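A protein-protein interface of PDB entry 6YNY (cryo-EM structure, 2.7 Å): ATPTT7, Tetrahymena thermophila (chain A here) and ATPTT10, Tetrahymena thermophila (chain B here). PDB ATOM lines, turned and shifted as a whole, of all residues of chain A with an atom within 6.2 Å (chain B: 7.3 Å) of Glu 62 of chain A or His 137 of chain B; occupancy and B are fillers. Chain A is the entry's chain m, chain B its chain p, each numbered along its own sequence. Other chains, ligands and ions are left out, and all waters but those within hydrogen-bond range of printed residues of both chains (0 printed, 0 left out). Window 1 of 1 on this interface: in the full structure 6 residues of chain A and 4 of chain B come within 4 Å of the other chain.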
ATOM      1  N   THR A  59      14.225  22.354 -20.612  1.00  0.00           N
ATOM      2  CA  THR A  59      13.334  22.489 -19.471  1.00  0.00           C
ATOM      3  C   THR A  59      12.380  23.665 -19.607  1.00  0.00           C
ATOM      4  O   THR A  59      11.623  23.943 -18.672  1.00  0.00           O
ATOM      5  CB  THR A  59      14.145  22.633 -18.184  1.00  0.00           C
ATOM      6  OG1 THR A  59      14.845  23.881 -18.188  1.00  0.00           O
ATOM      7  CG2 THR A  59      15.147  21.505 -18.067  1.00  0.00           C
ATOM      8  N   ASP A  60      12.400  24.358 -20.737  1.00  0.00           N
ATOM      9  CA  ASP A  60      11.460  25.439 -20.960  1.00  0.00           C
ATOM     10  C   ASP A  60      10.043  24.878 -21.078  1.00  0.00           C
ATOM     11  O   ASP A  60       9.833  23.859 -21.741  1.00  0.00           O
ATOM     12  CB  ASP A  60      11.832  26.210 -22.225  1.00  0.00           C
ATOM     13  CG  ASP A  60      10.978  27.440 -22.439  1.00  0.00           C
ATOM     14  OD1 ASP A  60       9.740  27.344 -22.332  1.00  0.00           O
ATOM     15  OD2 ASP A  60      11.550  28.512 -22.721  1.00  0.00           O
ATOM     16  N   PRO A  61       9.054  25.513 -20.444  1.00  0.00           N
ATOM     17  CA  PRO A  61       7.673  25.027 -20.576  1.00  0.00           C
ATOM     18  C   PRO A  61       7.180  24.953 -22.006  1.00  0.00           C
ATOM     19  O   PRO A  61       6.189  24.261 -22.265  1.00  0.00           O
ATOM     20  CB  PRO A  61       6.868  26.048 -19.764  1.00  0.00           C
ATOM     21  CG  PRO A  61       7.829  26.597 -18.801  1.00  0.00           C
ATOM     22  CD  PRO A  61       9.149  26.618 -19.478  1.00  0.00           C
ATOM     23  N   GLU A  62       7.832  25.641 -22.942  1.00  0.00           N
ATOM     24  CA  GLU A  62       7.399  25.588 -24.332  1.00  0.00           C
ATOM     25  C   GLU A  62       7.403  24.165 -24.867  1.00  0.00           C
ATOM     26  O   GLU A  62       6.550  23.808 -25.687  1.00  0.00           O
ATOM     27  CB  GLU A  62       8.299  26.475 -25.187  1.00  0.00           C
ATOM     28  CG  GLU A  62       7.938  26.491 -26.653  1.00  0.00           C
ATOM     29  CD  GLU A  62       8.849  27.378 -27.467  1.00  0.00           C
ATOM     30  OE1 GLU A  62       9.797  27.946 -26.890  1.00  0.00           O
ATOM     31  OE2 GLU A  62       8.615  27.511 -28.686  1.00  0.00           O
ATOM     32  N   TRP A  63       8.342  23.341 -24.417  1.00  0.00           N
ATOM     33  CA  TRP A  63       8.500  21.987 -24.920  1.00  0.00           C
ATOM     34  C   TRP A  63       7.709  20.966 -24.117  1.00  0.00           C
ATOM     35  O   TRP A  63       7.950  19.764 -24.253  1.00  0.00           O
ATOM     36  CB  TRP A  63       9.983  21.613 -24.935  1.00  0.00           C
ATOM     37  CG  TRP A  63      10.848  22.741 -25.382  1.00  0.00           C
ATOM     38  CD1 TRP A  63      11.853  23.325 -24.681  1.00  0.00           C
ATOM     39  CD2 TRP A  63      10.768  23.441 -26.627  1.00  0.00           C
ATOM     40  NE1 TRP A  63      12.412  24.341 -25.410  1.00  0.00           N
ATOM     41  CE2 TRP A  63      11.763  24.432 -26.612  1.00  0.00           C
ATOM     42  CE3 TRP A  63       9.956  23.323 -27.755  1.00  0.00           C
ATOM     43  CZ2 TRP A  63      11.967  25.297 -27.675  1.00  0.00           C
ATOM     44  CZ3 TRP A  63      10.161  24.180 -28.808  1.00  0.00           C
ATOM     45  CH2 TRP A  63      11.156  25.155 -28.763  1.00  0.00           C
ATOM     46  N   ASP A  64       6.772  21.416 -23.288  1.00  0.00           N
ATOM     47  CA  ASP A  64       5.881  20.521 -22.566  1.00  0.00           C
ATOM     48  C   ASP A  64       4.769  19.974 -23.445  1.00  0.00           C
ATOM     49  O   ASP A  64       3.932  19.208 -22.955  1.00  0.00           O
ATOM     50  CB  ASP A  64       5.277  21.242 -21.361  1.00  0.00           C
ATOM     51  CG  ASP A  64       6.284  21.482 -20.259  1.00  0.00           C
ATOM     52  OD1 ASP A  64       7.476  21.174 -20.461  1.00  0.00           O
ATOM     53  OD2 ASP A  64       5.882  21.972 -19.185  1.00  0.00           O
ATOM     54  N   ASP A  65       4.738  20.348 -24.723  1.00  0.00           N
ATOM     55  CA  ASP A  65       3.699  19.856 -25.616  1.00  0.00           C
ATOM     56  C   ASP A  65       3.832  18.361 -25.865  1.00  0.00           C
ATOM     57  O   ASP A  65       2.836  17.697 -26.172  1.00  0.00           O
ATOM     58  CB  ASP A  65       3.744  20.624 -26.935  1.00  0.00           C
ATOM     59  CG  ASP A  65       5.096  20.544 -27.619  1.00  0.00           C
ATOM     60  OD1 ASP A  65       5.504  19.432 -28.014  1.00  0.00           O
ATOM     61  OD2 ASP A  65       5.746  21.597 -27.772  1.00  0.00           O
ATOM     62  N   ASP A  66       5.040  17.816 -25.739  1.00  0.00           N
ATOM     63  CA  ASP A  66       5.282  16.396 -25.974  1.00  0.00           C
ATOM     64  C   ASP A  66       4.750  15.975 -27.340  1.00  0.00           C
ATOM     65  O   ASP A  66       4.109  14.936 -27.494  1.00  0.00           O
ATOM     66  CB  ASP A  66       4.670  15.547 -24.862  1.00  0.00           C
ATOM     67  CG  ASP A  66       5.373  15.735 -23.532  1.00  0.00           C
ATOM     68  OD1 ASP A  66       6.307  16.559 -23.464  1.00  0.00           O
ATOM     69  OD2 ASP A  66       4.998  15.054 -22.557  1.00  0.00           O
ATOM     70  N   TYR A 139       6.175  24.912 -39.341  1.00  0.00           N
ATOM     71  CA  TYR A 139       6.162  25.541 -38.026  1.00  0.00           C
ATOM     72  C   TYR A 139       7.551  25.551 -37.403  1.00  0.00           C
ATOM     73  O   TYR A 139       7.991  26.573 -36.868  1.00  0.00           O
ATOM     74  CB  TYR A 139       5.174  24.819 -37.112  1.00  0.00           C
ATOM     75  CG  TYR A 139       5.117  25.391 -35.720  1.00  0.00           C
ATOM     76  CD1 TYR A 139       4.384  26.530 -35.453  1.00  0.00           C
ATOM     77  CD2 TYR A 139       5.796  24.792 -34.675  1.00  0.00           C
ATOM     78  CE1 TYR A 139       4.331  27.058 -34.190  1.00  0.00           C
ATOM     79  CE2 TYR A 139       5.748  25.315 -33.408  1.00  0.00           C
ATOM     80  CZ  TYR A 139       5.015  26.447 -33.171  1.00  0.00           C
ATOM     81  OH  TYR A 139       4.966  26.970 -31.904  1.00  0.00           O
ATOM     82  N   ARG A 143       9.166  28.903 -36.227  1.00  0.00           N
ATOM     83  CA  ARG A 143       9.436  29.084 -34.807  1.00  0.00           C
ATOM     84  C   ARG A 143      10.929  29.130 -34.525  1.00  0.00           C
ATOM     85  O   ARG A 143      11.363  29.804 -33.585  1.00  0.00           O
ATOM     86  CB  ARG A 143       8.770  27.968 -34.005  1.00  0.00           C
ATOM     87  CG  ARG A 143       9.029  28.013 -32.518  1.00  0.00           C
ATOM     88  CD  ARG A 143       8.608  29.331 -31.918  1.00  0.00           C
ATOM     89  NE  ARG A 143       8.889  29.399 -30.493  1.00  0.00           N
ATOM     90  CZ  ARG A 143       8.898  30.526 -29.793  1.00  0.00           C
ATOM     91  NH1 ARG A 143       8.648  31.679 -30.390  1.00  0.00           N
ATOM     92  NH2 ARG A 143       9.164  30.502 -28.498  1.00  0.00           N
ATOM     93  N   LEU A 147      13.245  32.245 -32.547  1.00  0.00           N
ATOM     94  CA  LEU A 147      14.106  32.026 -31.394  1.00  0.00           C
ATOM     95  C   LEU A 147      15.537  32.461 -31.664  1.00  0.00           C
ATOM     96  O   LEU A 147      16.262  32.812 -30.728  1.00  0.00           O
ATOM     97  CB  LEU A 147      14.060  30.557 -30.996  1.00  0.00           C
ATOM     98  CG  LEU A 147      12.708  30.121 -30.446  1.00  0.00           C
ATOM     99  CD1 LEU A 147      12.599  28.626 -30.412  1.00  0.00           C
ATOM    100  CD2 LEU A 147      12.518  30.691 -29.061  1.00  0.00           C
ATOM    101  N   TYR B 121      -4.836  27.788 -28.404  1.00  0.00           N
ATOM    102  CA  TYR B 121      -3.882  27.050 -27.596  1.00  0.00           C
ATOM    103  C   TYR B 121      -3.652  27.776 -26.282  1.00  0.00           C
ATOM    104  O   TYR B 121      -3.533  29.004 -26.247  1.00  0.00           O
ATOM    105  CB  TYR B 121      -2.560  26.884 -28.341  1.00  0.00           C
ATOM    106  CG  TYR B 121      -1.606  25.917 -27.692  1.00  0.00           C
ATOM    107  CD1 TYR B 121      -1.690  24.562 -27.951  1.00  0.00           C
ATOM    108  CD2 TYR B 121      -0.620  26.357 -26.828  1.00  0.00           C
ATOM    109  CE1 TYR B 121      -0.824  23.672 -27.367  1.00  0.00           C
ATOM    110  CE2 TYR B 121       0.252  25.472 -26.238  1.00  0.00           C
ATOM    111  CZ  TYR B 121       0.146  24.131 -26.511  1.00  0.00           C
ATOM    112  OH  TYR B 121       1.013  23.245 -25.925  1.00  0.00           O
ATOM    113  N   PHE B 123      -2.124  27.047 -21.907  1.00  0.00           N
ATOM    114  CA  PHE B 123      -1.381  26.214 -20.981  1.00  0.00           C
ATOM    115  C   PHE B 123      -1.759  26.605 -19.564  1.00  0.00           C
ATOM    116  O   PHE B 123      -2.360  27.653 -19.322  1.00  0.00           O
ATOM    117  CB  PHE B 123       0.127  26.349 -21.199  1.00  0.00           C
ATOM    118  CG  PHE B 123       0.723  27.567 -20.569  1.00  0.00           C
ATOM    119  CD1 PHE B 123       0.288  28.828 -20.919  1.00  0.00           C
ATOM    120  CD2 PHE B 123       1.731  27.451 -19.635  1.00  0.00           C
ATOM    121  CE1 PHE B 123       0.837  29.942 -20.343  1.00  0.00           C
ATOM    122  CE2 PHE B 123       2.283  28.565 -19.058  1.00  0.00           C
ATOM    123  CZ  PHE B 123       1.836  29.813 -19.414  1.00  0.00           C
ATOM    124  N   LEU B 124      -1.403  25.739 -18.623  1.00  0.00           N
ATOM    125  CA  LEU B 124      -1.661  25.973 -17.209  1.00  0.00           C
ATOM    126  C   LEU B 124      -0.429  26.637 -16.611  1.00  0.00           C
ATOM    127  O   LEU B 124       0.615  25.998 -16.450  1.00  0.00           O
ATOM    128  CB  LEU B 124      -1.996  24.665 -16.505  1.00  0.00           C
ATOM    129  CG  LEU B 124      -3.078  23.837 -17.197  1.00  0.00           C
ATOM    130  CD1 LEU B 124      -3.345  22.557 -16.452  1.00  0.00           C
ATOM    131  CD2 LEU B 124      -4.348  24.631 -17.330  1.00  0.00           C
ATOM    132  N   ASP B 125      -0.551  27.919 -16.284  1.00  0.00           N
ATOM    133  CA  ASP B 125       0.583  28.718 -15.836  1.00  0.00           C
ATOM    134  C   ASP B 125       0.909  28.375 -14.388  1.00  0.00           C
ATOM    135  O   ASP B 125       0.122  28.658 -13.481  1.00  0.00           O
ATOM    136  CB  ASP B 125       0.270  30.201 -15.992  1.00  0.00           C
ATOM    137  CG  ASP B 125       1.484  31.078 -15.793  1.00  0.00           C
ATOM    138  OD1 ASP B 125       2.559  30.542 -15.452  1.00  0.00           O
ATOM    139  OD2 ASP B 125       1.364  32.307 -15.982  1.00  0.00           O
ATOM    140  N   ASP B 126       2.077  27.769 -14.170  1.00  0.00           N
ATOM    141  CA  ASP B 126       2.496  27.439 -12.815  1.00  0.00           C
ATOM    142  C   ASP B 126       2.643  28.688 -11.959  1.00  0.00           C
ATOM    143  O   ASP B 126       2.368  28.653 -10.755  1.00  0.00           O
ATOM    144  CB  ASP B 126       3.816  26.670 -12.849  1.00  0.00           C
ATOM    145  CG  ASP B 126       3.767  25.473 -13.770  1.00  0.00           C
ATOM    146  OD1 ASP B 126       2.714  25.256 -14.405  1.00  0.00           O
ATOM    147  OD2 ASP B 126       4.781  24.750 -13.860  1.00  0.00           O
ATOM    148  N   ASP B 127       3.074  29.793 -12.559  1.00  0.00           N
ATOM    149  CA  ASP B 127       3.296  31.036 -11.835  1.00  0.00           C
ATOM    150  C   ASP B 127       2.007  31.782 -11.528  1.00  0.00           C
ATOM    151  O   ASP B 127       2.067  32.883 -10.971  1.00  0.00           O
ATOM    152  CB  ASP B 127       4.230  31.941 -12.638  1.00  0.00           C
ATOM    153  CG  ASP B 127       5.521  31.252 -13.021  1.00  0.00           C
ATOM    154  OD1 ASP B 127       5.486  30.363 -13.896  1.00  0.00           O
ATOM    155  OD2 ASP B 127       6.574  31.596 -12.448  1.00  0.00           O
ATOM    156  N   LEU B 134      -3.489  32.207 -22.188  1.00  0.00           N
ATOM    157  CA  LEU B 134      -3.164  32.280 -23.604  1.00  0.00           C
ATOM    158  C   LEU B 134      -1.725  32.705 -23.846  1.00  0.00           C
ATOM    159  O   LEU B 134      -1.189  32.441 -24.927  1.00  0.00           O
ATOM    160  CB  LEU B 134      -4.096  33.263 -24.305  1.00  0.00           C
ATOM    161  CG  LEU B 134      -5.581  32.921 -24.334  1.00  0.00           C
ATOM    162  CD1 LEU B 134      -6.366  34.091 -24.861  1.00  0.00           C
ATOM    163  CD2 LEU B 134      -5.834  31.703 -25.183  1.00  0.00           C
ATOM    164  N   ASN B 135      -1.094  33.354 -22.870  1.00  0.00           N
ATOM    165  CA  ASN B 135       0.258  33.883 -23.024  1.00  0.00           C
ATOM    166  C   ASN B 135       1.272  32.770 -22.769  1.00  0.00           C
ATOM    167  O   ASN B 135       2.051  32.789 -21.813  1.00  0.00           O
ATOM    168  CB  ASN B 135       0.473  35.059 -22.083  1.00  0.00           C
ATOM    169  CG  ASN B 135      -0.713  35.998 -22.043  1.00  0.00           C
ATOM    170  OD1 ASN B 135      -1.194  36.362 -20.972  1.00  0.00           O
ATOM    171  ND2 ASN B 135      -1.196  36.391 -23.210  1.00  0.00           N
ATOM    172  N   HIS B 136       1.250  31.778 -23.651  1.00  0.00           N
ATOM    173  CA  HIS B 136       2.168  30.662 -23.516  1.00  0.00           C
ATOM    174  C   HIS B 136       3.565  31.062 -23.977  1.00  0.00           C
ATOM    175  O   HIS B 136       3.775  32.098 -24.611  1.00  0.00           O
ATOM    176  CB  HIS B 136       1.661  29.444 -24.286  1.00  0.00           C
ATOM    177  CG  HIS B 136       1.344  29.714 -25.720  1.00  0.00           C
ATOM    178  ND1 HIS B 136       2.306  29.728 -26.706  1.00  0.00           N
ATOM    179  CD2 HIS B 136       0.168  29.968 -26.338  1.00  0.00           C
ATOM    180  CE1 HIS B 136       1.736  29.985 -27.868  1.00  0.00           C
ATOM    181  NE2 HIS B 136       0.441  30.136 -27.673  1.00  0.00           N
ATOM    182  N   HIS B 137       4.534  30.215 -23.643  1.00  0.00           N
ATOM    183  CA  HIS B 137       5.943  30.518 -23.847  1.00  0.00           C
ATOM    184  C   HIS B 137       6.345  30.571 -25.310  1.00  0.00           C
ATOM    185  O   HIS B 137       7.511  30.860 -25.597  1.00  0.00           O
ATOM    186  CB  HIS B 137       6.792  29.490 -23.107  1.00  0.00           C
ATOM    187  CG  HIS B 137       6.676  29.582 -21.620  1.00  0.00           C
ATOM    188  ND1 HIS B 137       5.502  29.323 -20.948  1.00  0.00           N
ATOM    189  CD2 HIS B 137       7.584  29.921 -20.675  1.00  0.00           C
ATOM    190  CE1 HIS B 137       5.694  29.491 -19.652  1.00  0.00           C
ATOM    191  NE2 HIS B 137       6.949  29.853 -19.461  1.00  0.00           N
ATOM    192  N   ALA B 138       5.428  30.303 -26.233  1.00  0.00           N
ATOM    193  CA  ALA B 138       5.676  30.463 -27.657  1.00  0.00           C
ATOM    194  C   ALA B 138       4.996  31.699 -28.227  1.00  0.00           C
ATOM    195  O   ALA B 138       5.021  31.903 -29.444  1.00  0.00           O
ATOM    196  CB  ALA B 138       5.220  29.216 -28.408  1.00  0.00           C
ATOM    197  N   VAL B 139       4.395  32.522 -27.379  1.00  0.00           N
ATOM    198  CA  VAL B 139       3.754  33.755 -27.815  1.00  0.00           C
ATOM    199  C   VAL B 139       4.806  34.836 -28.004  1.00  0.00           C
ATOM    200  O   VAL B 139       5.826  34.871 -27.308  1.00  0.00           O
ATOM    201  CB  VAL B 139       2.682  34.186 -26.796  1.00  0.00           C
ATOM    202  CG1 VAL B 139       2.089  35.515 -27.177  1.00  0.00           C
ATOM    203  CG2 VAL B 139       1.605  33.142 -26.705  1.00  0.00           C
ATOM    204  N   THR B 140       4.556  35.728 -28.962  1.00  0.00           N
ATOM    205  CA  THR B 140       5.494  36.795 -29.290  1.00  0.00           C
ATOM    206  C   THR B 140       4.905  38.181 -29.066  1.00  0.00           C
ATOM    207  O   THR B 140       5.446  38.946 -28.263  1.00  0.00           O
ATOM    208  CB  THR B 140       5.962  36.648 -30.743  1.00  0.00           C
ATOM    209  OG1 THR B 140       4.831  36.662 -31.620  1.00  0.00           O
ATOM    210  CG2 THR B 140       6.727  35.354 -30.930  1.00  0.00           C
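Among the printed residues, pairs that only touch across the chains: Pro 61 of chain A with His 137 of chain B (3.4 Å), Arg 143 of chain A with Ala 138 of chain B (3.6 Å), Asp 60 of chain A with His 137 of chain B (3.7 Å), Glu 62 of chain A with Ala 138 of chain B (3.8 Å), Asp 65 of chain A with Tyr 121 of chain B (3.9 Å) and Glu 62 of chain A with His 137 of chain B (3.9 Å).
NH2 of Arg 143 of chain A sits at hydrogen-bond distance from O of His 137 of chain B (3.4 Å).
Of the 11 printed residues of chain A, 5 touch a printed residue of chain B. Printed residues of chain A that touch a printed residue of chain B: Asp 60, Pro 61, Glu 62, Asp 65 and Arg 143. Hydrophobic or aromatic side chains of chain A that line the printed part of chain B: Pro 61. Hydrophobic or aromatic side chains of chain B within 4 Å of the printed part of chain A: Tyr 121, His 137 and Ala 138. Among the printed residues, 7 pairs touch across the chains. Among the printed residues, no Asp or Glu carboxylate lies within 4 Å of a Lys or Arg side-chain nitrogen of the other chain.
The guanidinium group (NE) of Arg 143 of chain A lies within salt-bridge range of the side-chain carboxylate (OE2) of Glu 62 of chain A, 2.6 Å away. The backbone NH (N) of Ala 138 of chain B sits close to a ring nitrogen (ND1) of His 136 of chain B (3.2 Å). The backbone NH (N) of Glu 62 of chain A lies within hydrogen-bond range of the side-chain carboxylate (OD1) of Asp 60 of chain A (2.6 Å).
Of the printed residues of chain B, Asp 60 of chain A touches His 137 (3.7 Å). Of the printed residues of chain B, Pro 61 of chain A touches His 137 (3.4 Å). Of chain B, only His 137 (3.9 Å) and Ala 138 (3.8 Å) come within 4 Å of Glu 62 of chain A. Of the printed residues of chain B, Asp 65 of chain A touches Tyr 121 (3.9 Å). Printed residues of chain B within 4 Å of Arg 143 of chain A: His 137 and Ala 138. Leu 134 of chain B touches none of the printed residues of chain A. His 137 of chain B touches just these residues of chain A: Asp 60 (3.7 Å), Pro 61 (3.4 Å), Glu 62 (3.9 Å) and Arg 143 (3.4 Å). Of the printed residues of chain A, Ala 138 of chain B touches Glu 62 (3.8 Å) and Arg 143 (3.6 Å). The nearest residue of chain B that does not touch Glu 62 of chain A is Tyr 121 of chain B (5.6 Å). The nearest residue of chain A that does not touch His 137 of chain B is Leu 147 of chain A (6.1 Å). The nearest printed residue of chain B that does not touch Asp 65 of chain A is Ala 138 of chain B (7.7 Å).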
